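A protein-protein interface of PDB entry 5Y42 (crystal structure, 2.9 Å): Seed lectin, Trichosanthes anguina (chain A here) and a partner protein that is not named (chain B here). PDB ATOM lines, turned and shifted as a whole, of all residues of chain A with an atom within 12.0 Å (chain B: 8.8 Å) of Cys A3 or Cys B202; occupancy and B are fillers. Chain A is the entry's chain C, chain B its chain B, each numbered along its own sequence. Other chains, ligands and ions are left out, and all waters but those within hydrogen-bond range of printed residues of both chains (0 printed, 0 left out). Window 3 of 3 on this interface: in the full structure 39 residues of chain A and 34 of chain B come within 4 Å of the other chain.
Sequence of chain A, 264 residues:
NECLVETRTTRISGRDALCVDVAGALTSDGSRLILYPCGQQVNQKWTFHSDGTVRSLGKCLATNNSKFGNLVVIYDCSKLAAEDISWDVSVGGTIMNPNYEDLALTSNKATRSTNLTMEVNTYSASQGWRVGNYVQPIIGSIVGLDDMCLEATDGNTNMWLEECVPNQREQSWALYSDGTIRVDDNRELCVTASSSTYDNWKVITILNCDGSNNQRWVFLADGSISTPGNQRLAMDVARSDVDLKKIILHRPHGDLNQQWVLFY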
ATOM      1  N   ASN A   1       1.544  -5.586 -25.350  1.00  0.00           N
ATOM      2  CA  ASN A   1       2.907  -5.910 -24.847  1.00  0.00           C
ATOM      3  C   ASN A   1       3.948  -5.755 -25.944  1.00  0.00           C
ATOM      4  O   ASN A   1       3.931  -6.514 -26.913  1.00  0.00           O
ATOM      5  CB  ASN A   1       2.861  -7.351 -24.287  1.00  0.00           C
ATOM      6  CG  ASN A   1       2.432  -7.402 -22.824  1.00  0.00           C
ATOM      7  OD1 ASN A   1       2.739  -6.500 -22.029  1.00  0.00           O
ATOM      8  ND2 ASN A   1       1.727  -8.470 -22.464  1.00  0.00           N
ATOM      9  N   GLU A   2       4.869  -4.809 -25.768  1.00  0.00           N
ATOM     10  CA  GLU A   2       5.706  -4.315 -26.856  1.00  0.00           C
ATOM     11  C   GLU A   2       7.015  -3.803 -26.283  1.00  0.00           C
ATOM     12  O   GLU A   2       7.041  -3.375 -25.148  1.00  0.00           O
ATOM     13  CB  GLU A   2       4.958  -3.184 -27.571  1.00  0.00           C
ATOM     14  CG  GLU A   2       5.633  -2.497 -28.719  1.00  0.00           C
ATOM     15  CD  GLU A   2       5.955  -3.433 -29.848  1.00  0.00           C
ATOM     16  OE1 GLU A   2       6.958  -4.202 -29.751  1.00  0.00           O
ATOM     17  OE2 GLU A   2       5.206  -3.346 -30.845  1.00  0.00           O
ATOM     18  N   CYS A   3       8.092  -3.906 -27.045  1.00  0.00           N
ATOM     19  CA  CYS A   3       9.398  -3.667 -26.494  1.00  0.00           C
ATOM     20  C   CYS A   3       9.838  -2.247 -26.706  1.00  0.00           C
ATOM     21  O   CYS A   3      10.996  -1.907 -26.460  1.00  0.00           O
ATOM     22  CB  CYS A   3      10.375  -4.708 -27.057  1.00  0.00           C
ATOM     23  SG  CYS A   3       9.964  -6.408 -26.530  1.00  0.00           S
ATOM     24  N   LEU A   4       8.920  -1.422 -27.196  1.00  0.00           N
ATOM     25  CA  LEU A   4       9.145   0.023 -27.221  1.00  0.00           C
ATOM     26  C   LEU A   4       8.127   0.690 -26.331  1.00  0.00           C
ATOM     27  O   LEU A   4       6.953   0.437 -26.537  1.00  0.00           O
ATOM     28  CB  LEU A   4       8.932   0.601 -28.616  1.00  0.00           C
ATOM     29  CG  LEU A   4       9.724  -0.233 -29.602  1.00  0.00           C
ATOM     30  CD1 LEU A   4       9.019  -0.361 -30.937  1.00  0.00           C
ATOM     31  CD2 LEU A   4      11.113   0.339 -29.715  1.00  0.00           C
ATOM     32  N   VAL A   5       8.603   1.492 -25.356  1.00  0.00           N
ATOM     33  CA  VAL A   5       7.797   2.237 -24.457  1.00  0.00           C
ATOM     34  C   VAL A   5       8.049   3.703 -24.802  1.00  0.00           C
ATOM     35  O   VAL A   5       9.208   4.200 -24.826  1.00  0.00           O
ATOM     36  CB  VAL A   5       8.196   1.963 -23.021  1.00  0.00           C
ATOM     37  CG1 VAL A   5       7.172   2.572 -22.092  1.00  0.00           C
ATOM     38  CG2 VAL A   5       8.330   0.468 -22.779  1.00  0.00           C
ATOM     39  N   GLU A   6       6.957   4.422 -25.030  1.00  0.00           N
ATOM     40  CA  GLU A   6       7.062   5.807 -25.520  1.00  0.00           C
ATOM     41  C   GLU A   6       7.183   6.833 -24.407  1.00  0.00           C
ATOM     42  O   GLU A   6       8.123   7.657 -24.401  1.00  0.00           O
ATOM     43  CB  GLU A   6       5.891   6.139 -26.429  1.00  0.00           C
ATOM     44  CG  GLU A   6       5.941   5.373 -27.741  1.00  0.00           C
ATOM     45  CD  GLU A   6       7.060   5.822 -28.692  1.00  0.00           C
ATOM     46  OE1 GLU A   6       7.672   6.910 -28.519  1.00  0.00           O
ATOM     47  OE2 GLU A   6       7.331   5.056 -29.642  1.00  0.00           O
ATOM     48  N   THR A   7       6.171   6.858 -23.531  1.00  0.00           N
ATOM     49  CA  THR A   7       6.196   7.651 -22.305  1.00  0.00           C
ATOM     50  C   THR A   7       5.701   6.853 -21.080  1.00  0.00           C
ATOM     51  O   THR A   7       4.919   5.942 -21.204  1.00  0.00           O
ATOM     52  CB  THR A   7       5.348   8.937 -22.405  1.00  0.00           C
ATOM     53  OG1 THR A   7       3.976   8.637 -22.113  1.00  0.00           O
ATOM     54  CG2 THR A   7       5.474   9.582 -23.787  1.00  0.00           C
ATOM     55  N   ARG A   8       6.253   7.212 -19.929  1.00  0.00           N
ATOM     56  CA  ARG A   8       5.847   6.613 -18.650  1.00  0.00           C
ATOM     57  C   ARG A   8       5.809   7.591 -17.505  1.00  0.00           C
ATOM     58  O   ARG A   8       6.766   8.414 -17.377  1.00  0.00           O
ATOM     59  CB  ARG A   8       6.783   5.448 -18.363  1.00  0.00           C
ATOM     60  CG  ARG A   8       6.271   4.155 -19.006  1.00  0.00           C
ATOM     61  CD  ARG A   8       5.242   3.401 -18.172  1.00  0.00           C
ATOM     62  NE  ARG A   8       5.963   2.942 -16.998  1.00  0.00           N
ATOM     63  CZ  ARG A   8       5.870   3.464 -15.792  1.00  0.00           C
ATOM     64  NH1 ARG A   8       5.006   4.422 -15.526  1.00  0.00           N
ATOM     65  NH2 ARG A   8       6.636   2.997 -14.830  1.00  0.00           N
ATOM     66  N   SER A  50      10.404   9.604 -24.791  1.00  0.00           N
ATOM     67  CA  SER A  50      11.456   8.874 -25.525  1.00  0.00           C
ATOM     68  C   SER A  50      12.585   9.814 -26.019  1.00  0.00           C
ATOM     69  O   SER A  50      13.722   9.344 -26.280  1.00  0.00           O
ATOM     70  CB  SER A  50      10.885   8.062 -26.678  1.00  0.00           C
ATOM     71  OG  SER A  50      10.384   8.933 -27.664  1.00  0.00           O
ATOM     72  N   SER B 154      10.659 -10.631 -17.745  1.00  0.00           N
ATOM     73  CA  SER B 154      11.615 -10.647 -18.840  1.00  0.00           C
ATOM     74  C   SER B 154      11.240  -9.648 -19.945  1.00  0.00           C
ATOM     75  O   SER B 154      12.122  -8.918 -20.447  1.00  0.00           O
ATOM     76  CB  SER B 154      11.696 -12.014 -19.482  1.00  0.00           C
ATOM     77  OG  SER B 154      11.987 -12.988 -18.523  1.00  0.00           O
ATOM     78  N   LEU B 155       9.970  -9.619 -20.329  1.00  0.00           N
ATOM     79  CA  LEU B 155       9.502  -8.678 -21.368  1.00  0.00           C
ATOM     80  C   LEU B 155       9.742  -7.249 -20.939  1.00  0.00           C
ATOM     81  O   LEU B 155      10.220  -6.442 -21.740  1.00  0.00           O
ATOM     82  CB  LEU B 155       8.038  -8.913 -21.693  1.00  0.00           C
ATOM     83  CG  LEU B 155       7.348  -7.861 -22.569  1.00  0.00           C
ATOM     84  CD1 LEU B 155       8.076  -7.618 -23.889  1.00  0.00           C
ATOM     85  CD2 LEU B 155       5.910  -8.281 -22.819  1.00  0.00           C
ATOM     86  N   GLN B 156       9.386  -6.912 -19.703  1.00  0.00           N
ATOM     87  CA  GLN B 156       9.533  -5.542 -19.228  1.00  0.00           C
ATOM     88  C   GLN B 156      10.995  -5.119 -19.132  1.00  0.00           C
ATOM     89  O   GLN B 156      11.351  -3.973 -19.352  1.00  0.00           O
ATOM     90  CB  GLN B 156       8.843  -5.394 -17.879  1.00  0.00           C
ATOM     91  CG  GLN B 156       7.317  -5.522 -17.893  1.00  0.00           C
ATOM     92  CD  GLN B 156       6.612  -4.782 -19.031  1.00  0.00           C
ATOM     93  OE1 GLN B 156       6.963  -3.662 -19.372  1.00  0.00           O
ATOM     94  NE2 GLN B 156       5.615  -5.415 -19.613  1.00  0.00           N
ATOM     95  N   ILE B 157      11.854  -6.012 -18.758  1.00  0.00           N
ATOM     96  CA  ILE B 157      13.306  -5.737 -18.788  1.00  0.00           C
ATOM     97  C   ILE B 157      13.782  -5.378 -20.181  1.00  0.00           C
ATOM     98  O   ILE B 157      14.469  -4.412 -20.357  1.00  0.00           O
ATOM     99  CB  ILE B 157      14.079  -6.956 -18.252  1.00  0.00           C
ATOM    100  CG1 ILE B 157      13.817  -7.080 -16.742  1.00  0.00           C
ATOM    101  CG2 ILE B 157      15.574  -6.790 -18.491  1.00  0.00           C
ATOM    102  CD1 ILE B 157      14.373  -8.318 -16.075  1.00  0.00           C
ATOM    103  N   GLN B 158      13.401  -6.142 -21.169  1.00  0.00           N
ATOM    104  CA  GLN B 158      13.779  -5.796 -22.553  1.00  0.00           C
ATOM    105  C   GLN B 158      13.149  -4.518 -23.021  1.00  0.00           C
ATOM    106  O   GLN B 158      13.838  -3.691 -23.635  1.00  0.00           O
ATOM    107  CB  GLN B 158      13.476  -6.967 -23.468  1.00  0.00           C
ATOM    108  CG  GLN B 158      14.478  -8.076 -23.237  1.00  0.00           C
ATOM    109  CD  GLN B 158      13.878  -9.423 -23.423  1.00  0.00           C
ATOM    110  OE1 GLN B 158      13.225  -9.678 -24.439  1.00  0.00           O
ATOM    111  NE2 GLN B 158      14.078 -10.308 -22.435  1.00  0.00           N
ATOM    112  N   ALA B 159      11.883  -4.313 -22.668  1.00  0.00           N
ATOM    113  CA  ALA B 159      11.166  -3.116 -23.011  1.00  0.00           C
ATOM    114  C   ALA B 159      11.820  -1.875 -22.387  1.00  0.00           C
ATOM    115  O   ALA B 159      11.885  -0.798 -23.003  1.00  0.00           O
ATOM    116  CB  ALA B 159       9.757  -3.189 -22.502  1.00  0.00           C
ATOM    117  N   SER B 160      12.323  -2.035 -21.170  1.00  0.00           N
ATOM    118  CA  SER B 160      12.921  -0.943 -20.406  1.00  0.00           C
ATOM    119  C   SER B 160      14.155  -0.330 -21.010  1.00  0.00           C
ATOM    120  O   SER B 160      14.490   0.802 -20.693  1.00  0.00           O
ATOM    121  CB  SER B 160      13.248  -1.401 -19.000  1.00  0.00           C
ATOM    122  OG  SER B 160      14.411  -2.217 -19.009  1.00  0.00           O
ATOM    123  N   THR B 161      14.791  -1.038 -21.933  1.00  0.00           N
ATOM    124  CA  THR B 161      15.975  -0.506 -22.604  1.00  0.00           C
ATOM    125  C   THR B 161      15.663   0.699 -23.503  1.00  0.00           C
ATOM    126  O   THR B 161      16.546   1.446 -23.864  1.00  0.00           O
ATOM    127  CB  THR B 161      16.675  -1.599 -23.427  1.00  0.00           C
ATOM    128  OG1 THR B 161      15.771  -2.125 -24.406  1.00  0.00           O
ATOM    129  CG2 THR B 161      17.146  -2.726 -22.515  1.00  0.00           C
ATOM    130  N   SER B 162      14.404   0.837 -23.887  1.00  0.00           N
ATOM    131  CA  SER B 162      13.908   1.899 -24.770  1.00  0.00           C
ATOM    132  C   SER B 162      13.515   3.139 -24.012  1.00  0.00           C
ATOM    133  O   SER B 162      13.248   4.171 -24.628  1.00  0.00           O
ATOM    134  CB  SER B 162      12.721   1.373 -25.576  1.00  0.00           C
ATOM    135  OG  SER B 162      11.612   1.123 -24.746  1.00  0.00           O
ATOM    136  N   LEU B 163      13.390   3.088 -22.688  1.00  0.00           N
ATOM    137  CA  LEU B 163      13.012   4.273 -21.921  1.00  0.00           C
ATOM    138  C   LEU B 163      13.614   4.320 -20.528  1.00  0.00           C
ATOM    139  O   LEU B 163      12.876   4.284 -19.542  1.00  0.00           O
ATOM    140  CB  LEU B 163      11.476   4.361 -21.890  1.00  0.00           C
ATOM    141  CG  LEU B 163      10.815   5.661 -21.377  1.00  0.00           C
ATOM    142  CD1 LEU B 163      11.019   6.818 -22.334  1.00  0.00           C
ATOM    143  CD2 LEU B 163       9.319   5.491 -21.117  1.00  0.00           C
ATOM    144  N   LEU B 166      12.637   2.153 -17.333  1.00  0.00           N
ATOM    145  CA  LEU B 166      11.244   2.086 -16.939  1.00  0.00           C
ATOM    146  C   LEU B 166      10.482   1.021 -17.720  1.00  0.00           C
ATOM    147  O   LEU B 166      10.657   0.843 -18.906  1.00  0.00           O
ATOM    148  CB  LEU B 166      10.550   3.416 -17.194  1.00  0.00           C
ATOM    149  CG  LEU B 166      11.044   4.535 -16.291  1.00  0.00           C
ATOM    150  CD1 LEU B 166      10.644   5.908 -16.788  1.00  0.00           C
ATOM    151  CD2 LEU B 166      10.465   4.361 -14.900  1.00  0.00           C
ATOM    152  N   GLY B 168       7.130  -0.927 -19.326  1.00  0.00           N
ATOM    153  CA  GLY B 168       5.950  -0.576 -20.094  1.00  0.00           C
ATOM    154  C   GLY B 168       4.696  -0.882 -19.297  1.00  0.00           C
ATOM    155  O   GLY B 168       3.642  -0.303 -19.558  1.00  0.00           O
ATOM    156  N   GLN B 198      16.595 -14.636 -18.082  1.00  0.00           N
ATOM    157  CA  GLN B 198      15.393 -14.013 -18.645  1.00  0.00           C
ATOM    158  C   GLN B 198      15.008 -14.652 -19.986  1.00  0.00           C
ATOM    159  O   GLN B 198      15.855 -15.046 -20.817  1.00  0.00           O
ATOM    160  CB  GLN B 198      15.485 -12.472 -18.692  1.00  0.00           C
ATOM    161  CG  GLN B 198      16.613 -11.971 -19.538  1.00  0.00           C
ATOM    162  CD  GLN B 198      16.606 -10.484 -19.656  1.00  0.00           C
ATOM    163  OE1 GLN B 198      15.559  -9.873 -19.893  1.00  0.00           O
ATOM    164  NE2 GLN B 198      17.777  -9.881 -19.513  1.00  0.00           N
ATOM    165  N   LEU B 199      13.697 -14.756 -20.165  1.00  0.00           N
ATOM    166  CA  LEU B 199      13.109 -15.185 -21.422  1.00  0.00           C
ATOM    167  C   LEU B 199      13.335 -14.162 -22.519  1.00  0.00           C
ATOM    168  O   LEU B 199      13.140 -12.979 -22.323  1.00  0.00           O
ATOM    169  CB  LEU B 199      11.615 -15.387 -21.239  1.00  0.00           C
ATOM    170  CG  LEU B 199      10.827 -16.048 -22.343  1.00  0.00           C
ATOM    171  CD1 LEU B 199      11.553 -17.283 -22.800  1.00  0.00           C
ATOM    172  CD2 LEU B 199       9.436 -16.405 -21.831  1.00  0.00           C
ATOM    173  N   TYR B 200      13.796 -14.623 -23.672  1.00  0.00           N
ATOM    174  CA  TYR B 200      13.914 -13.772 -24.870  1.00  0.00           C
ATOM    175  C   TYR B 200      12.553 -13.318 -25.427  1.00  0.00           C
ATOM    176  O   TYR B 200      11.682 -14.156 -25.675  1.00  0.00           O
ATOM    177  CB  TYR B 200      14.693 -14.477 -26.012  1.00  0.00           C
ATOM    178  CG  TYR B 200      14.750 -13.629 -27.276  1.00  0.00           C
ATOM    179  CD1 TYR B 200      15.692 -12.594 -27.407  1.00  0.00           C
ATOM    180  CD2 TYR B 200      13.850 -13.825 -28.318  1.00  0.00           C
ATOM    181  CE1 TYR B 200      15.741 -11.798 -28.551  1.00  0.00           C
ATOM    182  CE2 TYR B 200      13.889 -13.035 -29.462  1.00  0.00           C
ATOM    183  CZ  TYR B 200      14.825 -12.011 -29.564  1.00  0.00           C
ATOM    184  OH  TYR B 200      14.865 -11.210 -30.674  1.00  0.00           O
ATOM    185  N   HIS B 201      12.374 -12.032 -25.618  1.00  0.00           N
ATOM    186  CA  HIS B 201      11.190 -11.515 -26.319  1.00  0.00           C
ATOM    187  C   HIS B 201      11.601 -10.717 -27.548  1.00  0.00           C
ATOM    188  O   HIS B 201      11.104 -10.944 -28.667  1.00  0.00           O
ATOM    189  CB  HIS B 201      10.321 -10.649 -25.382  1.00  0.00           C
ATOM    190  CG  HIS B 201       9.524 -11.414 -24.371  1.00  0.00           C
ATOM    191  ND1 HIS B 201       8.285 -11.943 -24.649  1.00  0.00           N
ATOM    192  CD2 HIS B 201       9.774 -11.696 -23.071  1.00  0.00           C
ATOM    193  CE1 HIS B 201       7.812 -12.537 -23.566  1.00  0.00           C
ATOM    194  NE2 HIS B 201       8.698 -12.407 -22.596  1.00  0.00           N
ATOM    195  N   CYS B 202      12.543  -9.786 -27.320  1.00  0.00           N
ATOM    196  CA  CYS B 202      12.948  -8.807 -28.342  1.00  0.00           C
ATOM    197  C   CYS B 202      14.442  -8.567 -28.388  1.00  0.00           C
ATOM    198  O   CYS B 202      15.136  -8.769 -27.396  1.00  0.00           O
ATOM    199  CB  CYS B 202      12.285  -7.464 -28.108  1.00  0.00           C
ATOM    200  SG  CYS B 202      10.490  -7.574 -28.143  1.00  0.00           S
ATOM    201  N   GLN B 203      14.894  -8.142 -29.576  1.00  0.00           N
ATOM    202  CA  GLN B 203      16.295  -7.881 -29.881  1.00  0.00           C
ATOM    203  C   GLN B 203      16.666  -6.447 -29.460  1.00  0.00           C
ATOM    204  O   GLN B 203      16.528  -5.450 -30.218  1.00  0.00           O
ATOM    205  CB  GLN B 203      16.572  -8.116 -31.366  1.00  0.00           C
ATOM    206  CG  GLN B 203      18.016  -7.907 -31.839  1.00  0.00           C
ATOM    207  CD  GLN B 203      18.936  -9.113 -31.635  1.00  0.00           C
ATOM    208  OE1 GLN B 203      18.618 -10.004 -30.866  1.00  0.00           O
ATOM    209  NE2 GLN B 203      20.097  -9.124 -32.310  1.00  0.00           N
ATOM    210  N   VAL B 204      17.176  -6.353 -28.240  1.00  0.00           N
ATOM    211  CA  VAL B 204      17.489  -5.036 -27.609  1.00  0.00           C
ATOM    212  C   VAL B 204      18.913  -5.020 -27.029  1.00  0.00           C
ATOM    213  O   VAL B 204      19.597  -6.019 -27.172  1.00  0.00           O
ATOM    214  CB  VAL B 204      16.413  -4.667 -26.553  1.00  0.00           C
ATOM    215  CG1 VAL B 204      15.064  -4.347 -27.202  1.00  0.00           C
ATOM    216  CG2 VAL B 204      16.228  -5.782 -25.549  1.00  0.00           C
ATOM    217  N   SER B 205      19.350  -3.904 -26.407  1.00  0.00           N
ATOM    218  CA  SER B 205      20.718  -3.766 -25.835  1.00  0.00           C
ATOM    219  C   SER B 205      20.921  -2.643 -24.770  1.00  0.00           C
ATOM    220  O   SER B 205      20.237  -1.618 -24.816  1.00  0.00           O
ATOM    221  CB  SER B 205      21.675  -3.487 -26.981  1.00  0.00           C
ATOM    222  OG  SER B 205      21.274  -2.293 -27.626  1.00  0.00           O
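Among the printed residues, pairs that only touch across the chains: Asn A1 with Leu B155, Asn A1 with Gln B156, Glu A2 with Ala B159, Cys A3 with Leu B155, Cys A3 with Ala B159, Cys A3 with Ser B162, Leu A4 with Ser B162, Val A5 with Ala B159, Val A5 with Leu B163, Val A5 with Gly B168, Glu A6 with Leu B163, Thr A7 with Leu B163, Arg A8 with Leu B163 and Ser A50 with Leu B163.
Of the 20 printed residues of chain B, 7 touch a printed residue of chain A. Along chain B the printed residues that touch a printed residue of chain A span positions 155 to 202. Hydrophobic or aromatic side chains of chain A within 4 Å of the printed part of chain B: Val A5. Among the printed residues, 16 pairs touch across the chains.
Of chain B, only Leu B155 (3.5 Å), Ala B159 (3.7 Å), Ser B162 (3.5 Å) and Cys B202 (2.1 Å) come within 4 Å of Cys A3. Of chain A, only Cys A3 comes within 4 Å of Cys B202. Of chain B, only Ser B162 comes within 4 Å of Leu A4. Of the printed residues of chain A, Leu B155 touches Asn A1 (3.5 Å) and Cys A3 (3.5 Å). No residue of chain A comes within 4 Å of Gln B158. Of chain A, only Glu A2, Cys A3 and Val A5 come within 4 Å of Ala B159. No residue of chain A comes within 4 Å of Thr B161. Of the printed residues of chain A, Ser B162 touches Cys A3 (3.5 Å), Leu A4 (3.7 Å) and Val A5 (3.1 Å). No residue of chain A comes within 4 Å of Tyr B200. No residue of chain A comes within 4 Å of His B201. No residue of chain A comes within 4 Å of Gln B203. Of the printed residues of chain A, Leu B163 touches Val A5 (3.7 Å), Glu A6 (3.7 Å), Thr A7 (3.9 Å), Arg A8 (3.7 Å) and Ser A50 (3.8 Å). Printed residues of chain B within 4 Å of Arg A8: Leu B163 (3.7 Å). Printed residues of chain B within 4 Å of Asn A1: Leu B155 (3.5 Å) and Gln B156 (3.9 Å). Leu B166 touches none of the printed residues of chain A. The nearest residue of chain A that does not touch Cys B202 is Glu A2 (5.1 Å).
OE1 of Gln B156 is in hydrogen-bond range of N of Gly B168 (2.7 Å). OE1 of Gln B158 lies within hydrogen-bond range of N of Cys B202, 3.0 Å away. OG of Ser B162 lies within hydrogen-bond range of O of Ala B159 (2.6 Å). O of Glu A6 lies within hydrogen-bond range of N of Ser A50.
The side-chain hydroxyl (OG) of Ser B162 sits at hydrogen-bond distance from the backbone NH (N) of Val A5 (3.1 Å). The side-chain sulfur (SG) of Cys B202 forms a disulfide with the side-chain sulfur (SG) of Cys A3 (2.1 Å).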
